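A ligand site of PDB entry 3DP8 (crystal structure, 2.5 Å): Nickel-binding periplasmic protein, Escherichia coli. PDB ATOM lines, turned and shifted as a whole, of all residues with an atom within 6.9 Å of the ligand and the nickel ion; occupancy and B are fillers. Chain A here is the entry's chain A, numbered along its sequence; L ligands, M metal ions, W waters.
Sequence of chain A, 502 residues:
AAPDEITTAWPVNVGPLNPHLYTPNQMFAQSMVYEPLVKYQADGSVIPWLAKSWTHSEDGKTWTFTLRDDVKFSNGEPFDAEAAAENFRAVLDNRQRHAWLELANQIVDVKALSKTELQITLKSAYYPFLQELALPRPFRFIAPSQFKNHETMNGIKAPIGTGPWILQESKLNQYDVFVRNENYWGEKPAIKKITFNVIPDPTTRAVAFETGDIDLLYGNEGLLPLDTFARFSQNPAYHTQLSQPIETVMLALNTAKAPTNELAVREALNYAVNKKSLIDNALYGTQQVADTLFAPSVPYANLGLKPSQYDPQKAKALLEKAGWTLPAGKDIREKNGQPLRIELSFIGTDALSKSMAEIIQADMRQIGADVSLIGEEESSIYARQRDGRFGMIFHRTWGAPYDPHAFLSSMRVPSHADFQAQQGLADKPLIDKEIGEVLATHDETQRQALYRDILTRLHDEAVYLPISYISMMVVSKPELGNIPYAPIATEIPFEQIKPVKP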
ATOM      1  N   LEU A  21      -1.466 -23.770  -3.461  1.00  0.00           N
ATOM      2  CA  LEU A  21      -1.501 -25.217  -3.649  1.00  0.00           C
ATOM      3  C   LEU A  21      -2.586 -25.893  -2.783  1.00  0.00           C
ATOM      4  O   LEU A  21      -3.306 -25.225  -2.056  1.00  0.00           O
ATOM      5  CB  LEU A  21      -0.118 -25.880  -3.422  1.00  0.00           C
ATOM      6  CG  LEU A  21       1.021 -25.569  -4.428  1.00  0.00           C
ATOM      7  CD1 LEU A  21       2.360 -26.258  -4.010  1.00  0.00           C
ATOM      8  CD2 LEU A  21       0.668 -25.879  -5.902  1.00  0.00           C
ATOM      9  N   TYR A  22      -2.684 -27.227  -2.882  1.00  0.00           N
ATOM     10  CA  TYR A  22      -3.763 -27.964  -2.269  1.00  0.00           C
ATOM     11  C   TYR A  22      -3.141 -28.833  -1.194  1.00  0.00           C
ATOM     12  O   TYR A  22      -2.373 -28.334  -0.362  1.00  0.00           O
ATOM     13  CB  TYR A  22      -4.594 -28.761  -3.356  1.00  0.00           C
ATOM     14  CG  TYR A  22      -5.147 -27.808  -4.425  1.00  0.00           C
ATOM     15  CD1 TYR A  22      -4.366 -27.438  -5.543  1.00  0.00           C
ATOM     16  CD2 TYR A  22      -6.379 -27.194  -4.250  1.00  0.00           C
ATOM     17  CE1 TYR A  22      -4.832 -26.516  -6.490  1.00  0.00           C
ATOM     18  CE2 TYR A  22      -6.857 -26.267  -5.194  1.00  0.00           C
ATOM     19  CZ  TYR A  22      -6.083 -25.940  -6.320  1.00  0.00           C
ATOM     20  OH  TYR A  22      -6.555 -25.019  -7.235  1.00  0.00           O
ATOM     21  N   THR A  23      -3.440 -30.130  -1.210  1.00  0.00           N
ATOM     22  CA  THR A  23      -3.020 -31.009  -0.160  1.00  0.00           C
ATOM     23  C   THR A  23      -1.480 -30.949  -0.069  1.00  0.00           C
ATOM     24  O   THR A  23      -0.817 -30.929  -1.094  1.00  0.00           O
ATOM     25  CB  THR A  23      -3.565 -32.435  -0.417  1.00  0.00           C
ATOM     26  OG1 THR A  23      -4.302 -32.858   0.742  1.00  0.00           O
ATOM     27  CG2 THR A  23      -2.442 -33.445  -0.733  1.00  0.00           C
ATOM     28  N   MET A  27      -7.538 -26.117   4.254  1.00  0.00           N
ATOM     29  CA  MET A  27      -8.223 -24.941   3.725  1.00  0.00           C
ATOM     30  C   MET A  27      -8.657 -23.918   4.781  1.00  0.00           C
ATOM     31  O   MET A  27      -8.678 -22.699   4.548  1.00  0.00           O
ATOM     32  CB  MET A  27      -9.434 -25.314   2.821  1.00  0.00           C
ATOM     33  CG  MET A  27      -9.215 -26.309   1.635  1.00  0.00           C
ATOM     34  SD  MET A  27     -10.741 -26.500   0.565  1.00  0.00           S
ATOM     35  CE  MET A  27     -11.183 -24.805   0.570  1.00  0.00           C
ATOM     36  N   GLN A  30      -5.540 -21.868   5.420  1.00  0.00           N
ATOM     37  CA  GLN A  30      -5.278 -20.958   4.307  1.00  0.00           C
ATOM     38  C   GLN A  30      -6.190 -19.772   4.421  1.00  0.00           C
ATOM     39  O   GLN A  30      -5.776 -18.635   4.191  1.00  0.00           O
ATOM     40  CB  GLN A  30      -5.505 -21.679   2.963  1.00  0.00           C
ATOM     41  CG  GLN A  30      -4.327 -22.436   2.450  1.00  0.00           C
ATOM     42  CD  GLN A  30      -4.658 -23.460   1.386  1.00  0.00           C
ATOM     43  OE1 GLN A  30      -5.554 -24.291   1.580  1.00  0.00           O
ATOM     44  NE2 GLN A  30      -3.922 -23.436   0.274  1.00  0.00           N
ATOM     45  N   ARG A  97      -3.160 -27.437 -12.977  1.00  0.00           N
ATOM     46  CA  ARG A  97      -3.536 -27.930 -11.654  1.00  0.00           C
ATOM     47  C   ARG A  97      -4.877 -27.331 -11.206  1.00  0.00           C
ATOM     48  O   ARG A  97      -5.619 -28.001 -10.507  1.00  0.00           O
ATOM     49  CB  ARG A  97      -2.466 -27.538 -10.634  1.00  0.00           C
ATOM     50  CG  ARG A  97      -2.690 -27.975  -9.174  1.00  0.00           C
ATOM     51  CD  ARG A  97      -2.576 -29.531  -9.030  1.00  0.00           C
ATOM     52  NE  ARG A  97      -2.997 -30.036  -7.698  1.00  0.00           N
ATOM     53  CZ  ARG A  97      -4.261 -30.296  -7.329  1.00  0.00           C
ATOM     54  NH1 ARG A  97      -5.310 -30.096  -8.140  1.00  0.00           N
ATOM     55  NH2 ARG A  97      -4.496 -30.763  -6.118  1.00  0.00           N
ATOM     56  N   HIS A  98      -5.139 -26.064 -11.576  1.00  0.00           N
ATOM     57  CA  HIS A  98      -6.347 -25.335 -11.193  1.00  0.00           C
ATOM     58  C   HIS A  98      -7.504 -25.491 -12.209  1.00  0.00           C
ATOM     59  O   HIS A  98      -8.478 -24.693 -12.207  1.00  0.00           O
ATOM     60  CB  HIS A  98      -6.032 -23.867 -11.031  1.00  0.00           C
ATOM     61  CG  HIS A  98      -4.887 -23.594 -10.103  1.00  0.00           C
ATOM     62  ND1 HIS A  98      -4.613 -24.363  -8.988  1.00  0.00           N
ATOM     63  CD2 HIS A  98      -3.932 -22.637 -10.126  1.00  0.00           C
ATOM     64  CE1 HIS A  98      -3.548 -23.897  -8.386  1.00  0.00           C
ATOM     65  NE2 HIS A  98      -3.128 -22.827  -9.041  1.00  0.00           N
ATOM     66  N   TRP A 100      -9.845 -27.660 -12.668  1.00  0.00           N
ATOM     67  CA  TRP A 100     -11.068 -27.975 -11.978  1.00  0.00           C
ATOM     68  C   TRP A 100     -11.897 -26.710 -11.802  1.00  0.00           C
ATOM     69  O   TRP A 100     -13.092 -26.803 -11.786  1.00  0.00           O
ATOM     70  CB  TRP A 100     -10.772 -28.649 -10.600  1.00  0.00           C
ATOM     71  CG  TRP A 100     -10.164 -27.709  -9.589  1.00  0.00           C
ATOM     72  CD1 TRP A 100      -8.828 -27.450  -9.389  1.00  0.00           C
ATOM     73  CD2 TRP A 100     -10.875 -26.878  -8.667  1.00  0.00           C
ATOM     74  NE1 TRP A 100      -8.666 -26.525  -8.392  1.00  0.00           N
ATOM     75  CE2 TRP A 100      -9.899 -26.153  -7.919  1.00  0.00           C
ATOM     76  CE3 TRP A 100     -12.230 -26.708  -8.376  1.00  0.00           C
ATOM     77  CZ2 TRP A 100     -10.247 -25.231  -6.900  1.00  0.00           C
ATOM     78  CZ3 TRP A 100     -12.577 -25.793  -7.341  1.00  0.00           C
ATOM     79  CH2 TRP A 100     -11.571 -25.046  -6.636  1.00  0.00           C
ATOM     80  N   LEU A 135     -13.109 -17.783  -3.200  1.00  0.00           N
ATOM     81  CA  LEU A 135     -12.873 -19.112  -2.711  1.00  0.00           C
ATOM     82  C   LEU A 135     -11.631 -19.157  -1.785  1.00  0.00           C
ATOM     83  O   LEU A 135     -10.743 -18.301  -1.888  1.00  0.00           O
ATOM     84  CB  LEU A 135     -12.739 -20.086  -3.861  1.00  0.00           C
ATOM     85  CG  LEU A 135     -13.988 -20.515  -4.642  1.00  0.00           C
ATOM     86  CD1 LEU A 135     -13.515 -21.521  -5.653  1.00  0.00           C
ATOM     87  CD2 LEU A 135     -15.125 -21.143  -3.807  1.00  0.00           C
ATOM     88  N   PRO A 136     -11.582 -20.130  -0.859  1.00  0.00           N
ATOM     89  CA  PRO A 136     -10.405 -20.118   0.003  1.00  0.00           C
ATOM     90  C   PRO A 136      -9.099 -20.113  -0.827  1.00  0.00           C
ATOM     91  O   PRO A 136      -8.047 -19.689  -0.330  1.00  0.00           O
ATOM     92  CB  PRO A 136     -10.523 -21.441   0.789  1.00  0.00           C
ATOM     93  CG  PRO A 136     -12.001 -21.679   0.811  1.00  0.00           C
ATOM     94  CD  PRO A 136     -12.470 -21.270  -0.545  1.00  0.00           C
ATOM     95  N   ARG A 137      -9.176 -20.596  -2.062  1.00  0.00           N
ATOM     96  CA  ARG A 137      -7.995 -21.039  -2.797  1.00  0.00           C
ATOM     97  C   ARG A 137      -8.349 -21.433  -4.250  1.00  0.00           C
ATOM     98  O   ARG A 137      -9.372 -22.065  -4.484  1.00  0.00           O
ATOM     99  CB  ARG A 137      -7.276 -22.151  -2.022  1.00  0.00           C
ATOM    100  CG  ARG A 137      -7.707 -23.559  -2.283  1.00  0.00           C
ATOM    101  CD  ARG A 137      -6.977 -24.526  -1.388  1.00  0.00           C
ATOM    102  NE  ARG A 137      -7.443 -25.911  -1.511  1.00  0.00           N
ATOM    103  CZ  ARG A 137      -7.030 -26.937  -0.778  1.00  0.00           C
ATOM    104  NH1 ARG A 137      -6.098 -26.758   0.165  1.00  0.00           N
ATOM    105  NH2 ARG A 137      -7.535 -28.150  -0.953  1.00  0.00           N
ATOM    106  N   PRO A 138      -7.518 -21.023  -5.245  1.00  0.00           N
ATOM    107  CA  PRO A 138      -6.219 -20.352  -5.208  1.00  0.00           C
ATOM    108  C   PRO A 138      -6.108 -18.849  -5.360  1.00  0.00           C
ATOM    109  O   PRO A 138      -4.980 -18.342  -5.483  1.00  0.00           O
ATOM    110  CB  PRO A 138      -5.544 -20.961  -6.435  1.00  0.00           C
ATOM    111  CG  PRO A 138      -6.715 -21.024  -7.461  1.00  0.00           C
ATOM    112  CD  PRO A 138      -7.937 -21.320  -6.637  1.00  0.00           C
ATOM    113  N   ARG A 396     -16.822 -37.533  -1.565  1.00  0.00           N
ATOM    114  CA  ARG A 396     -17.838 -36.621  -1.091  1.00  0.00           C
ATOM    115  C   ARG A 396     -18.018 -35.340  -1.980  1.00  0.00           C
ATOM    116  O   ARG A 396     -17.143 -35.065  -2.807  1.00  0.00           O
ATOM    117  CB  ARG A 396     -17.518 -36.275   0.377  1.00  0.00           C
ATOM    118  CG  ARG A 396     -16.084 -35.842   0.641  1.00  0.00           C
ATOM    119  CD  ARG A 396     -15.873 -35.178   2.048  1.00  0.00           C
ATOM    120  NE  ARG A 396     -15.929 -36.195   3.074  1.00  0.00           N
ATOM    121  CZ  ARG A 396     -16.631 -36.087   4.193  1.00  0.00           C
ATOM    122  NH1 ARG A 396     -16.605 -37.099   5.054  1.00  0.00           N
ATOM    123  NH2 ARG A 396     -17.387 -35.003   4.440  1.00  0.00           N
ATOM    124  N   THR A 397     -19.123 -34.574  -1.824  1.00  0.00           N
ATOM    125  CA  THR A 397     -19.268 -33.297  -2.567  1.00  0.00           C
ATOM    126  C   THR A 397     -18.606 -32.194  -1.716  1.00  0.00           C
ATOM    127  O   THR A 397     -18.064 -32.510  -0.694  1.00  0.00           O
ATOM    128  CB  THR A 397     -20.760 -32.902  -2.907  1.00  0.00           C
ATOM    129  OG1 THR A 397     -21.501 -32.681  -1.701  1.00  0.00           O
ATOM    130  CG2 THR A 397     -21.448 -33.914  -3.749  1.00  0.00           C
ATOM    131  N   TRP A 398     -18.664 -30.925  -2.091  1.00  0.00           N
ATOM    132  CA  TRP A 398     -17.795 -29.939  -1.416  1.00  0.00           C
ATOM    133  C   TRP A 398     -18.403 -28.890  -0.563  1.00  0.00           C
ATOM    134  O   TRP A 398     -17.653 -28.106   0.027  1.00  0.00           O
ATOM    135  CB  TRP A 398     -16.944 -29.189  -2.438  1.00  0.00           C
ATOM    136  CG  TRP A 398     -15.943 -30.062  -3.202  1.00  0.00           C
ATOM    137  CD1 TRP A 398     -15.402 -31.246  -2.780  1.00  0.00           C
ATOM    138  CD2 TRP A 398     -15.384 -29.804  -4.488  1.00  0.00           C
ATOM    139  NE1 TRP A 398     -14.550 -31.733  -3.733  1.00  0.00           N
ATOM    140  CE2 TRP A 398     -14.512 -30.870  -4.786  1.00  0.00           C
ATOM    141  CE3 TRP A 398     -15.520 -28.760  -5.411  1.00  0.00           C
ATOM    142  CZ2 TRP A 398     -13.778 -30.930  -5.980  1.00  0.00           C
ATOM    143  CZ3 TRP A 398     -14.794 -28.801  -6.582  1.00  0.00           C
ATOM    144  CH2 TRP A 398     -13.920 -29.883  -6.848  1.00  0.00           C
ATOM    145  N   GLY A 399     -19.744 -28.794  -0.526  1.00  0.00           N
ATOM    146  CA  GLY A 399     -20.424 -27.826   0.328  1.00  0.00           C
ATOM    147  C   GLY A 399     -20.599 -26.517  -0.430  1.00  0.00           C
ATOM    148  O   GLY A 399     -19.958 -26.302  -1.463  1.00  0.00           O
ATOM    149  N   TYR A 402     -19.451 -24.477  -3.652  1.00  0.00           N
ATOM    150  CA  TYR A 402     -18.977 -25.288  -4.732  1.00  0.00           C
ATOM    151  C   TYR A 402     -20.084 -26.128  -5.350  1.00  0.00           C
ATOM    152  O   TYR A 402     -19.972 -26.512  -6.532  1.00  0.00           O
ATOM    153  CB  TYR A 402     -17.892 -26.234  -4.250  1.00  0.00           C
ATOM    154  CG  TYR A 402     -16.682 -25.590  -3.623  1.00  0.00           C
ATOM    155  CD1 TYR A 402     -16.653 -25.302  -2.258  1.00  0.00           C
ATOM    156  CD2 TYR A 402     -15.546 -25.343  -4.382  1.00  0.00           C
ATOM    157  CE1 TYR A 402     -15.522 -24.749  -1.686  1.00  0.00           C
ATOM    158  CE2 TYR A 402     -14.442 -24.775  -3.840  1.00  0.00           C
ATOM    159  CZ  TYR A 402     -14.425 -24.485  -2.493  1.00  0.00           C
ATOM    160  OH  TYR A 402     -13.282 -23.922  -2.001  1.00  0.00           O
ATOM    161  N   SER A 410     -15.407 -29.531 -12.120  1.00  0.00           N
ATOM    162  CA  SER A 410     -14.258 -30.391 -11.832  1.00  0.00           C
ATOM    163  C   SER A 410     -14.412 -31.783 -12.433  1.00  0.00           C
ATOM    164  O   SER A 410     -13.397 -32.493 -12.652  1.00  0.00           O
ATOM    165  CB  SER A 410     -14.070 -30.536 -10.323  1.00  0.00           C
ATOM    166  OG  SER A 410     -14.681 -31.742  -9.883  1.00  0.00           O
ATOM    167  N   SER A 415      -7.884 -35.708 -14.543  1.00  0.00           N
ATOM    168  CA  SER A 415      -7.834 -36.231 -13.195  1.00  0.00           C
ATOM    169  C   SER A 415      -8.400 -35.419 -11.993  1.00  0.00           C
ATOM    170  O   SER A 415      -7.887 -34.318 -11.615  1.00  0.00           O
ATOM    171  CB  SER A 415      -6.464 -36.828 -12.849  1.00  0.00           C
ATOM    172  OG  SER A 415      -6.581 -37.790 -11.791  1.00  0.00           O
ATOM    173  N   HIS A 416      -9.550 -35.922 -11.554  1.00  0.00           N
ATOM    174  CA  HIS A 416      -9.648 -36.711 -10.291  1.00  0.00           C
ATOM    175  C   HIS A 416     -10.768 -37.718 -10.401  1.00  0.00           C
ATOM    176  O   HIS A 416     -11.008 -38.256 -11.499  1.00  0.00           O
ATOM    177  CB  HIS A 416      -9.499 -36.021  -8.887  1.00  0.00           C
ATOM    178  CG  HIS A 416      -9.976 -34.615  -8.801  1.00  0.00           C
ATOM    179  ND1 HIS A 416     -10.712 -34.149  -7.729  1.00  0.00           N
ATOM    180  CD2 HIS A 416      -9.780 -33.544  -9.625  1.00  0.00           C
ATOM    181  CE1 HIS A 416     -10.973 -32.858  -7.898  1.00  0.00           C
ATOM    182  NE2 HIS A 416     -10.431 -32.473  -9.045  1.00  0.00           N
ATOM    183  N   THR A 490     -15.960 -24.907   4.189  1.00  0.00           N
ATOM    184  CA  THR A 490     -14.578 -25.298   4.537  1.00  0.00           C
ATOM    185  C   THR A 490     -13.872 -24.323   5.496  1.00  0.00           C
ATOM    186  O   THR A 490     -12.880 -24.702   6.146  1.00  0.00           O
ATOM    187  CB  THR A 490     -13.664 -25.516   3.277  1.00  0.00           C
ATOM    188  OG1 THR A 490     -13.742 -24.360   2.415  1.00  0.00           O
ATOM    189  CG2 THR A 490     -14.094 -26.789   2.493  1.00  0.00           C
HETATM  190  C1  LIG L   1      -8.791 -30.197  -5.821  1.00  0.00           C
HETATM  191  C2  LIG L   1     -10.232 -29.568  -5.475  1.00  0.00           C
HETATM  192  C3  LIG L   1     -10.526 -28.177  -4.731  1.00  0.00           C
HETATM  193  C4  LIG L   1     -11.980 -28.212  -4.117  1.00  0.00           C
HETATM  194  C5  LIG L   1     -12.057 -29.400  -3.100  1.00  0.00           C
HETATM  195  C6  LIG L   1     -12.867 -29.245  -1.827  1.00  0.00           C
HETATM  196  C7  LIG L   1      -9.755 -27.743  -3.451  1.00  0.00           C
HETATM  197  O1  LIG L   1      -8.055 -30.601  -4.875  1.00  0.00           O
HETATM  198  O2  LIG L   1      -8.470 -30.358  -7.049  1.00  0.00           O
HETATM  199  O3  LIG L   1     -12.841 -30.233  -1.057  1.00  0.00           O
HETATM  200  O4  LIG L   1     -13.495 -28.175  -1.646  1.00  0.00           O
HETATM  201  O5  LIG L   1      -9.695 -26.506  -3.165  1.00  0.00           O
HETATM  202  O6  LIG L   1      -9.365 -28.674  -2.732  1.00  0.00           O
HETATM  203 NI    NI M   1     -10.367 -30.522  -3.156  1.00  0.00          NI
HETATM  204  O   HOH W   1     -10.962 -24.019  -3.639  1.00  0.00           O
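NE of Arg 137 is in salt-bridge range of O5 of the ligand, 2.9 Å away. The guanidinium group (NH1) of Arg 97 lies within salt-bridge range of an oxygen (O2) of the ligand, at 3.4 Å.
The side-chain amide oxygen (OE1) of Gln 30 is in hydrogen-bond range of the guanidinium group (NH1) of Arg 137 (2.9 Å). The side-chain hydroxyl of Tyr 22 lies within hydrogen-bond range of the indole nitrogen of Trp 100. ND1 of His 98 lies within hydrogen-bond range of OH of Tyr 22, 2.7 Å away.
CE2 of Tyr 22 touches O5 of the ligand, at 3.5 Å. SD of Met 27 touches O5 of the ligand (3.9 Å). Trp 100 touches the ligand. Trp 398 touches the ligand (CD1 to O3, 3.2 Å). Tyr 402 touches the ligand (CZ to O4, 3.9 Å). His 416 touches the ligand (NE2 to O2, 3.5 Å). Hydrophobic or aromatic side chains within 4 Å of the ligand: Tyr 22, Met 27, Trp 100, Trp 398, Tyr 402 and His 416. Of the 21 residues printed, 8 come within 4 Å of the ligand.
No residue comes within 4 Å of the nickel ion. The nearest printed residue that does not touch the nickel ion is Arg 137 (4.3 Å).
An oxygen (O6) of the ligand binds the nickel ion (2.1 Å). The nickel ion has one donor atom within binding distance.
Water W1 lies within hydrogen-bond range of the backbone carbonyl oxygen (O) of Arg 137 (2.7 Å), an oxygen (O5) of the ligand (2.8 Å) and the side-chain hydroxyl (OH) of Tyr 402 (2.8 Å).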
